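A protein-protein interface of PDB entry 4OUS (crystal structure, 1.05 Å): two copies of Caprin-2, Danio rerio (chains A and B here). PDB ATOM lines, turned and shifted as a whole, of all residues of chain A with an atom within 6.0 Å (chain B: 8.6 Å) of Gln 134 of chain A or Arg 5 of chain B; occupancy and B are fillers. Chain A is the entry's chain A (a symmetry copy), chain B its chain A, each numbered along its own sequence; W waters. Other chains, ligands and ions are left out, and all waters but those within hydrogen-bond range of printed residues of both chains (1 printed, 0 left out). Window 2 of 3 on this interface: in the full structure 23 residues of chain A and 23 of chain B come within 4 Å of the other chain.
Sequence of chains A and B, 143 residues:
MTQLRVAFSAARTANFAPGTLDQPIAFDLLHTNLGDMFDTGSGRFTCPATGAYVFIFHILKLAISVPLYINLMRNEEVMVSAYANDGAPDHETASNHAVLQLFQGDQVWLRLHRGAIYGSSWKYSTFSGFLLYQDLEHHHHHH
The side-chain hydroxyl (OH) of Tyr 133 of chain A is in hydrogen-bond range of the backbone NH (N) of Val 6 of chain B (3.1 Å).
NH2 of Arg 5 of chain B sits at hydrogen-bond distance from O of Gln 134 of chain A, at 2.4 Å.
The backbone carbonyl oxygen of Ala 7 of chain B sits at hydrogen-bond distance from the backbone NH of Leu 34 of chain B, 2.8 Å away.
The backbone carbonyl oxygen (O) of Ala 52 of chain A is in hydrogen-bond range of the backbone NH (N) of Leu 132 of chain A (2.8 Å).
The backbone NH (N) of Ala 52 of chain A is in hydrogen-bond range of the backbone carbonyl oxygen (O) of Tyr 133 of chain A (2.8 Å).
N of Leu 4 of chain A is in hydrogen-bond range of OE1 of Gln 134 of chain A, 3.1 Å away.
N of Leu 4 of chain B sits at hydrogen-bond distance from OE1 of Gln 134 of chain B (3.1 Å).
O of Val 6 of chain B sits at hydrogen-bond distance from N of Leu 131 of chain B.
Among the printed residues, pairs that only touch across the chains: Leu 132 of chain A with Ala 7 of chain B (3.9 Å), Leu 132 of chain A with Phe 130 of chain B (3.7 Å), Tyr 133 of chain A with Leu 4 of chain B (3.7 Å), Tyr 133 of chain A with Arg 5 of chain B (3.5 Å), Tyr 133 of chain A with Leu 34 of chain B (3.8 Å), Tyr 133 of chain A with Leu 131 of chain B (3.7 Å) and Asp 135 of chain A with Arg 5 of chain B (3.997 Å).
Ala 49 of chain A touches none of the printed residues of chain B.
Of chain B, only Leu 4, Arg 5, Val 6, Leu 34 and Leu 131 come within 4 Å of Tyr 133 of chain A.
Gln 134 of chain A touches just one residue of chain B: Arg 5.
Of the printed residues of chain B, Asp 135 of chain A touches Arg 5 (3.997 Å).
Printed residues of chain A within 4 Å of Leu 4 of chain B: Tyr 133 (3.7 Å).
Printed residues of chain A within 4 Å of Ala 7 of chain B: Leu 132.
Printed residues of chain A within 4 Å of Phe 130 of chain B: Leu 132.
Of the printed residues of chain A, Leu 131 of chain B touches Tyr 133 (3.7 Å).
The nearest printed residue of chain A that does not touch Arg 5 of chain B is Gly 51 of chain A (6.3 Å).
The nearest printed residue of chain A that does not touch Leu 4 of chain B is Leu 132 of chain A (8.1 Å).
Of the 10 printed residues of chain A, 4 touch a printed residue of chain B.
Printed residues of chain A that touch a printed residue of chain B: Leu 132, Tyr 133, Gln 134 and Asp 135.
Printed residues of chain B that touch a printed residue of chain A: Leu 4, Arg 5, Val 6, Ala 7, Leu 34, Phe 130 and Leu 131.
Among the printed residues, no Asp or Glu carboxylate lies within 4 Å of a Lys or Arg side-chain nitrogen of the other chain.
Positions printed for both chains: 4, 49, 131 and 134.
Water W1 lies within hydrogen-bond range of the backbone carbonyl oxygen of Leu 131 of chain B and the side-chain hydroxyl of Tyr 133 of chain A.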
ATOM      1  N   LEU A   4     -34.483 -29.524  24.482  1.00  0.00           N
ATOM      2  CA  LEU A   4     -33.750 -30.285  25.486  1.00  0.00           C
ATOM      3  C   LEU A   4     -33.162 -29.375  26.559  1.00  0.00           C
ATOM      4  O   LEU A   4     -32.772 -28.244  26.277  1.00  0.00           O
ATOM      5  CB  LEU A   4     -32.632 -31.099  24.828  1.00  0.00           C
ATOM      6  CG  LEU A   4     -32.748 -32.622  24.895  1.00  0.00           C
ATOM      7  CD1 LEU A   4     -31.714 -33.279  23.990  1.00  0.00           C
ATOM      8  CD2 LEU A   4     -32.598 -33.109  26.327  1.00  0.00           C
ATOM      9  N   ALA A  49     -27.325 -34.061  21.507  1.00  0.00           N
ATOM     10  CA  ALA A  49     -27.987 -33.385  20.407  1.00  0.00           C
ATOM     11  C   ALA A  49     -27.040 -32.364  19.820  1.00  0.00           C
ATOM     12  O   ALA A  49     -26.442 -31.567  20.544  1.00  0.00           O
ATOM     13  CB  ALA A  49     -29.273 -32.719  20.874  1.00  0.00           C
ATOM     14  N   THR A  50     -26.886 -32.406  18.507  1.00  0.00           N
ATOM     15  CA  THR A  50     -26.017 -31.472  17.819  1.00  0.00           C
ATOM     16  C   THR A  50     -26.410 -30.046  18.193  1.00  0.00           C
ATOM     17  O   THR A  50     -27.595 -29.720  18.276  1.00  0.00           O
ATOM     18  CB  THR A  50     -26.088 -31.715  16.308  1.00  0.00           C
ATOM     19  OG1 THR A  50     -25.584 -33.032  16.046  1.00  0.00           O
ATOM     20  CG2 THR A  50     -25.274 -30.695  15.533  1.00  0.00           C
ATOM     21  N   GLY A  51     -25.412 -29.220  18.487  1.00  0.00           N
ATOM     22  CA  GLY A  51     -25.669 -27.858  18.903  1.00  0.00           C
ATOM     23  C   GLY A  51     -24.438 -27.197  19.484  1.00  0.00           C
ATOM     24  O   GLY A  51     -23.353 -27.779  19.487  1.00  0.00           O
ATOM     25  N   ALA A  52     -24.614 -25.971  19.968  1.00  0.00           N
ATOM     26  CA  ALA A  52     -23.539 -25.206  20.583  1.00  0.00           C
ATOM     27  C   ALA A  52     -23.637 -25.353  22.093  1.00  0.00           C
ATOM     28  O   ALA A  52     -24.717 -25.196  22.666  1.00  0.00           O
ATOM     29  CB  ALA A  52     -23.613 -23.746  20.178  1.00  0.00           C
ATOM     30  N   LEU A 131     -25.996 -26.710  27.328  1.00  0.00           N
ATOM     31  CA  LEU A 131     -26.492 -26.482  25.988  1.00  0.00           C
ATOM     32  C   LEU A 131     -26.877 -25.020  25.818  1.00  0.00           C
ATOM     33  O   LEU A 131     -27.652 -24.481  26.612  1.00  0.00           O
ATOM     34  CB  LEU A 131     -27.689 -27.391  25.729  1.00  0.00           C
ATOM     35  CG  LEU A 131     -28.457 -27.196  24.430  1.00  0.00           C
ATOM     36  CD1 LEU A 131     -27.578 -27.446  23.219  1.00  0.00           C
ATOM     37  CD2 LEU A 131     -29.657 -28.122  24.419  1.00  0.00           C
ATOM     38  N   LEU A 132     -26.327 -24.380  24.795  1.00  0.00           N
ATOM     39  CA  LEU A 132     -26.670 -23.004  24.462  1.00  0.00           C
ATOM     40  C   LEU A 132     -27.702 -22.954  23.327  1.00  0.00           C
ATOM     41  O   LEU A 132     -28.768 -22.355  23.473  1.00  0.00           O
ATOM     42  CB  LEU A 132     -25.411 -22.226  24.083  1.00  0.00           C
ATOM     43  CG  LEU A 132     -25.615 -20.771  23.664  1.00  0.00           C
ATOM     44  CD1 LEU A 132     -26.150 -19.942  24.826  1.00  0.00           C
ATOM     45  CD2 LEU A 132     -24.311 -20.193  23.138  1.00  0.00           C
ATOM     46  N   TYR A 133     -27.377 -23.588  22.204  1.00  0.00           N
ATOM     47  CA  TYR A 133     -28.272 -23.654  21.049  1.00  0.00           C
ATOM     48  C   TYR A 133     -28.416 -25.065  20.538  1.00  0.00           C
ATOM     49  O   TYR A 133     -27.431 -25.672  20.133  1.00  0.00           O
ATOM     50  CB  TYR A 133     -27.760 -22.803  19.895  1.00  0.00           C
ATOM     51  CG  TYR A 133     -27.688 -21.341  20.176  1.00  0.00           C
ATOM     52  CD1 TYR A 133     -28.826 -20.638  20.535  1.00  0.00           C
ATOM     53  CD2 TYR A 133     -26.492 -20.648  20.045  1.00  0.00           C
ATOM     54  CE1 TYR A 133     -28.773 -19.288  20.779  1.00  0.00           C
ATOM     55  CE2 TYR A 133     -26.426 -19.305  20.292  1.00  0.00           C
ATOM     56  CZ  TYR A 133     -27.569 -18.629  20.656  1.00  0.00           C
ATOM     57  OH  TYR A 133     -27.499 -17.281  20.897  1.00  0.00           O
ATOM     58  N   GLN A 134     -29.638 -25.578  20.511  1.00  0.00           N
ATOM     59  CA  GLN A 134     -29.874 -26.898  19.943  1.00  0.00           C
ATOM     60  C   GLN A 134     -30.122 -26.786  18.443  1.00  0.00           C
ATOM     61  O   GLN A 134     -30.829 -25.887  17.992  1.00  0.00           O
ATOM     62  CB  GLN A 134     -31.056 -27.572  20.634  1.00  0.00           C
ATOM     63  CG  GLN A 134     -31.289 -29.006  20.198  1.00  0.00           C
ATOM     64  CD  GLN A 134     -32.491 -29.628  20.874  1.00  0.00           C
ATOM     65  OE1 GLN A 134     -33.126 -29.011  21.730  1.00  0.00           O
ATOM     66  NE2 GLN A 134     -32.812 -30.860  20.493  1.00  0.00           N
ATOM     67  N   ASP A 135     -29.543 -27.696  17.668  1.00  0.00           N
ATOM     68  CA  ASP A 135     -29.742 -27.681  16.225  1.00  0.00           C
ATOM     69  C   ASP A 135     -31.179 -28.047  15.875  1.00  0.00           C
ATOM     70  O   ASP A 135     -31.835 -28.791  16.605  1.00  0.00           O
ATOM     71  CB  ASP A 135     -28.775 -28.642  15.535  1.00  0.00           C
ATOM     72  CG  ASP A 135     -28.544 -28.289  14.084  1.00  0.00           C
ATOM     73  OD1 ASP A 135     -29.261 -28.826  13.213  1.00  0.00           O
ATOM     74  OD2 ASP A 135     -27.645 -27.467  13.816  1.00  0.00           O
ATOM     75  N   LEU B   4     -32.241 -14.868  17.114  1.00  0.00           N
ATOM     76  CA  LEU B   4     -30.870 -14.893  16.620  1.00  0.00           C
ATOM     77  C   LEU B   4     -30.004 -15.860  17.421  1.00  0.00           C
ATOM     78  O   LEU B   4     -30.199 -16.027  18.623  1.00  0.00           O
ATOM     79  CB  LEU B   4     -30.259 -13.489  16.666  1.00  0.00           C
ATOM     80  CG  LEU B   4     -29.897 -12.843  15.329  1.00  0.00           C
ATOM     81  CD1 LEU B   4     -29.545 -11.374  15.520  1.00  0.00           C
ATOM     82  CD2 LEU B   4     -28.751 -13.590  14.665  1.00  0.00           C
ATOM     83  N   ARG B   5     -29.056 -16.501  16.747  1.00  0.00           N
ATOM     84  CA  ARG B   5     -28.041 -17.292  17.426  1.00  0.00           C
ATOM     85  C   ARG B   5     -26.711 -16.582  17.262  1.00  0.00           C
ATOM     86  O   ARG B   5     -26.221 -16.419  16.145  1.00  0.00           O
ATOM     87  CB  ARG B   5     -27.986 -18.713  16.871  1.00  0.00           C
ATOM     88  CG  ARG B   5     -29.290 -19.470  17.063  1.00  0.00           C
ATOM     89  CD  ARG B   5     -29.173 -20.928  16.665  1.00  0.00           C
ATOM     90  NE  ARG B   5     -30.309 -21.701  17.158  1.00  0.00           N
ATOM     91  CZ  ARG B   5     -30.475 -23.003  16.952  1.00  0.00           C
ATOM     92  NH1 ARG B   5     -29.579 -23.687  16.254  1.00  0.00           N
ATOM     93  NH2 ARG B   5     -31.541 -23.622  17.442  1.00  0.00           N
ATOM     94  N   VAL B   6     -26.149 -16.117  18.371  1.00  0.00           N
ATOM     95  CA  VAL B   6     -24.937 -15.324  18.318  1.00  0.00           C
ATOM     96  C   VAL B   6     -23.981 -15.823  19.394  1.00  0.00           C
ATOM     97  O   VAL B   6     -24.290 -15.758  20.589  1.00  0.00           O
ATOM     98  CB  VAL B   6     -25.224 -13.823  18.537  1.00  0.00           C
ATOM     99  CG1 VAL B   6     -23.953 -13.007  18.353  1.00  0.00           C
ATOM    100  CG2 VAL B   6     -26.323 -13.327  17.605  1.00  0.00           C
ATOM    101  N   ALA B   7     -22.827 -16.335  18.979  1.00  0.00           N
ATOM    102  CA  ALA B   7     -21.832 -16.834  19.914  1.00  0.00           C
ATOM    103  C   ALA B   7     -20.498 -16.933  19.219  1.00  0.00           C
ATOM    104  O   ALA B   7     -20.428 -17.339  18.063  1.00  0.00           O
ATOM    105  CB  ALA B   7     -22.239 -18.195  20.468  1.00  0.00           C
ATOM    106  N   PHE B   8     -19.429 -16.577  19.919  1.00  0.00           N
ATOM    107  CA  PHE B   8     -18.094 -16.775  19.384  1.00  0.00           C
ATOM    108  C   PHE B   8     -17.196 -17.342  20.464  1.00  0.00           C
ATOM    109  O   PHE B   8     -17.437 -17.150  21.665  1.00  0.00           O
ATOM    110  CB  PHE B   8     -17.494 -15.476  18.820  1.00  0.00           C
ATOM    111  CG  PHE B   8     -17.163 -14.457  19.866  1.00  0.00           C
ATOM    112  CD1 PHE B   8     -15.896 -14.387  20.419  1.00  0.00           C
ATOM    113  CD2 PHE B   8     -18.126 -13.566  20.302  1.00  0.00           C
ATOM    114  CE1 PHE B   8     -15.608 -13.452  21.399  1.00  0.00           C
ATOM    115  CE2 PHE B   8     -17.841 -12.628  21.267  1.00  0.00           C
ATOM    116  CZ  PHE B   8     -16.580 -12.574  21.818  1.00  0.00           C
ATOM    117  N   ASN B  33     -18.347 -18.984  15.500  1.00  0.00           N
ATOM    118  CA  ASN B  33     -18.654 -17.589  15.218  1.00  0.00           C
ATOM    119  C   ASN B  33     -20.073 -17.493  14.656  1.00  0.00           C
ATOM    120  O   ASN B  33     -20.299 -16.955  13.571  1.00  0.00           O
ATOM    121  CB  ASN B  33     -17.621 -16.981  14.260  1.00  0.00           C
ATOM    122  CG  ASN B  33     -17.602 -15.452  14.287  1.00  0.00           C
ATOM    123  OD1 ASN B  33     -18.207 -14.811  15.148  1.00  0.00           O
ATOM    124  ND2 ASN B  33     -16.893 -14.864  13.334  1.00  0.00           N
ATOM    125  N   LEU B  34     -21.020 -18.050  15.405  1.00  0.00           N
ATOM    126  CA  LEU B  34     -22.436 -17.983  15.054  1.00  0.00           C
ATOM    127  C   LEU B  34     -22.872 -16.532  15.004  1.00  0.00           C
ATOM    128  O   LEU B  34     -22.682 -15.787  15.970  1.00  0.00           O
ATOM    129  CB  LEU B  34     -23.290 -18.750  16.062  1.00  0.00           C
ATOM    130  CG  LEU B  34     -23.020 -20.244  16.202  1.00  0.00           C
ATOM    131  CD1 LEU B  34     -23.860 -20.822  17.324  1.00  0.00           C
ATOM    132  CD2 LEU B  34     -23.301 -20.977  14.896  1.00  0.00           C
ATOM    133  N   GLY B  35     -23.430 -16.130  13.868  1.00  0.00           N
ATOM    134  CA  GLY B  35     -23.814 -14.747  13.657  1.00  0.00           C
ATOM    135  C   GLY B  35     -22.759 -13.902  12.962  1.00  0.00           C
ATOM    136  O   GLY B  35     -23.048 -12.775  12.559  1.00  0.00           O
ATOM    137  N   ASP B  36     -21.549 -14.441  12.818  1.00  0.00           N
ATOM    138  CA  ASP B  36     -20.459 -13.776  12.097  1.00  0.00           C
ATOM    139  C   ASP B  36     -20.071 -12.428  12.679  1.00  0.00           C
ATOM    140  O   ASP B  36     -19.623 -11.544  11.946  1.00  0.00           O
ATOM    141  CB  ASP B  36     -20.819 -13.576  10.621  1.00  0.00           C
ATOM    142  CG  ASP B  36     -21.249 -14.847   9.955  1.00  0.00           C
ATOM    143  OD1 ASP B  36     -20.360 -15.628   9.558  1.00  0.00           O
ATOM    144  OD2 ASP B  36     -22.474 -15.062   9.827  1.00  0.00           O
ATOM    145  N   MET B  37     -20.221 -12.258  13.983  1.00  0.00           N
ATOM    146  CA  MET B  37     -20.043 -10.939  14.572  1.00  0.00           C
ATOM    147  C   MET B  37     -18.684 -10.713  15.246  1.00  0.00           C
ATOM    148  O   MET B  37     -18.391  -9.586  15.659  1.00  0.00           O
ATOM    149  CB  MET B  37     -21.171 -10.664  15.573  1.00  0.00           C
ATOM    150  CG  MET B  37     -22.592 -10.708  14.994  1.00  0.00           C
ATOM    151  SD  MET B  37     -22.832  -9.855  13.430  1.00  0.00           S
ATOM    152  CE  MET B  37     -22.277  -8.256  13.905  1.00  0.00           C
ATOM    153  N   PHE B  45     -15.938  -7.934  18.902  1.00  0.00           N
ATOM    154  CA  PHE B  45     -17.296  -8.423  18.719  1.00  0.00           C
ATOM    155  C   PHE B  45     -18.225  -7.242  18.481  1.00  0.00           C
ATOM    156  O   PHE B  45     -18.216  -6.296  19.266  1.00  0.00           O
ATOM    157  CB  PHE B  45     -17.744  -9.195  19.958  1.00  0.00           C
ATOM    158  CG  PHE B  45     -19.196  -9.572  19.941  1.00  0.00           C
ATOM    159  CD1 PHE B  45     -19.633 -10.644  19.188  1.00  0.00           C
ATOM    160  CD2 PHE B  45     -20.123  -8.853  20.673  1.00  0.00           C
ATOM    161  CE1 PHE B  45     -20.969 -11.002  19.170  1.00  0.00           C
ATOM    162  CE2 PHE B  45     -21.462  -9.207  20.661  1.00  0.00           C
ATOM    163  CZ  PHE B  45     -21.883 -10.281  19.907  1.00  0.00           C
ATOM    164  N   PRO B  48     -25.068  -7.449  17.135  1.00  0.00           N
ATOM    165  CA  PRO B  48     -25.997  -7.421  15.997  1.00  0.00           C
ATOM    166  C   PRO B  48     -27.433  -7.091  16.386  1.00  0.00           C
ATOM    167  O   PRO B  48     -28.259  -6.837  15.511  1.00  0.00           O
ATOM    168  CB  PRO B  48     -25.923  -8.846  15.465  1.00  0.00           C
ATOM    169  CG  PRO B  48     -25.722  -9.664  16.702  1.00  0.00           C
ATOM    170  CD  PRO B  48     -24.827  -8.829  17.601  1.00  0.00           C
ATOM    171  N   ALA B  49     -27.723  -7.125  17.681  1.00  0.00           N
ATOM    172  CA  ALA B  49     -29.081  -6.954  18.164  1.00  0.00           C
ATOM    173  C   ALA B  49     -29.036  -6.585  19.628  1.00  0.00           C
ATOM    174  O   ALA B  49     -28.354  -7.233  20.422  1.00  0.00           O
ATOM    175  CB  ALA B  49     -29.896  -8.222  17.954  1.00  0.00           C
ATOM    176  N   TYR B  53     -25.682  -9.918  26.816  1.00  0.00           N
ATOM    177  CA  TYR B  53     -24.631 -10.796  26.314  1.00  0.00           C
ATOM    178  C   TYR B  53     -23.674 -11.177  27.437  1.00  0.00           C
ATOM    179  O   TYR B  53     -23.376 -10.351  28.299  1.00  0.00           O
ATOM    180  CB  TYR B  53     -23.852 -10.107  25.186  1.00  0.00           C
ATOM    181  CG  TYR B  53     -24.645  -9.894  23.912  1.00  0.00           C
ATOM    182  CD1 TYR B  53     -24.434 -10.700  22.803  1.00  0.00           C
ATOM    183  CD2 TYR B  53     -25.606  -8.891  23.815  1.00  0.00           C
ATOM    184  CE1 TYR B  53     -25.151 -10.521  21.633  1.00  0.00           C
ATOM    185  CE2 TYR B  53     -26.337  -8.706  22.645  1.00  0.00           C
ATOM    186  CZ  TYR B  53     -26.102  -9.527  21.554  1.00  0.00           C
ATOM    187  OH  TYR B  53     -26.805  -9.372  20.380  1.00  0.00           O
ATOM    188  N   GLY B 129     -18.018 -15.089  23.811  1.00  0.00           N
ATOM    189  CA  GLY B 129     -19.215 -14.365  24.164  1.00  0.00           C
ATOM    190  C   GLY B 129     -20.434 -14.998  23.537  1.00  0.00           C
ATOM    191  O   GLY B 129     -20.333 -15.688  22.515  1.00  0.00           O
ATOM    192  N   PHE B 130     -21.595 -14.769  24.136  1.00  0.00           N
ATOM    193  CA  PHE B 130     -22.822 -15.252  23.535  1.00  0.00           C
ATOM    194  C   PHE B 130     -24.011 -14.402  23.945  1.00  0.00           C
ATOM    195  O   PHE B 130     -24.022 -13.756  24.997  1.00  0.00           O
ATOM    196  CB  PHE B 130     -23.073 -16.733  23.871  1.00  0.00           C
ATOM    197  CG  PHE B 130     -23.166 -17.044  25.341  1.00  0.00           C
ATOM    198  CD1 PHE B 130     -24.378 -16.967  26.007  1.00  0.00           C
ATOM    199  CD2 PHE B 130     -22.056 -17.481  26.039  1.00  0.00           C
ATOM    200  CE1 PHE B 130     -24.472 -17.282  27.348  1.00  0.00           C
ATOM    201  CE2 PHE B 130     -22.146 -17.796  27.384  1.00  0.00           C
ATOM    202  CZ  PHE B 130     -23.358 -17.699  28.034  1.00  0.00           C
ATOM    203  N   LEU B 131     -25.017 -14.415  23.086  1.00  0.00           N
ATOM    204  CA  LEU B 131     -26.287 -13.770  23.338  1.00  0.00           C
ATOM    205  C   LEU B 131     -27.062 -14.542  24.394  1.00  0.00           C
ATOM    206  O   LEU B 131     -27.265 -15.752  24.261  1.00  0.00           O
ATOM    207  CB  LEU B 131     -27.081 -13.687  22.037  1.00  0.00           C
ATOM    208  CG  LEU B 131     -28.513 -13.181  22.114  1.00  0.00           C
ATOM    209  CD1 LEU B 131     -28.576 -11.759  22.636  1.00  0.00           C
ATOM    210  CD2 LEU B 131     -29.147 -13.274  20.740  1.00  0.00           C
ATOM    211  N   GLN B 134     -32.285 -11.636  23.776  1.00  0.00           N
ATOM    212  CA  GLN B 134     -32.466 -10.678  22.694  1.00  0.00           C
ATOM    213  C   GLN B 134     -33.627  -9.743  23.013  1.00  0.00           C
ATOM    214  O   GLN B 134     -34.665 -10.180  23.506  1.00  0.00           O
ATOM    215  CB  GLN B 134     -32.709 -11.404  21.374  1.00  0.00           C
ATOM    216  CG  GLN B 134     -32.774 -10.485  20.169  1.00  0.00           C
ATOM    217  CD  GLN B 134     -33.054 -11.234  18.884  1.00  0.00           C
ATOM    218  OE1 GLN B 134     -33.135 -12.463  18.873  1.00  0.00           O
ATOM    219  NE2 GLN B 134     -33.201 -10.496  17.790  1.00  0.00           N
HETATM  220  O   HOH W   1     -29.162 -16.967  22.977  1.00  0.00           O
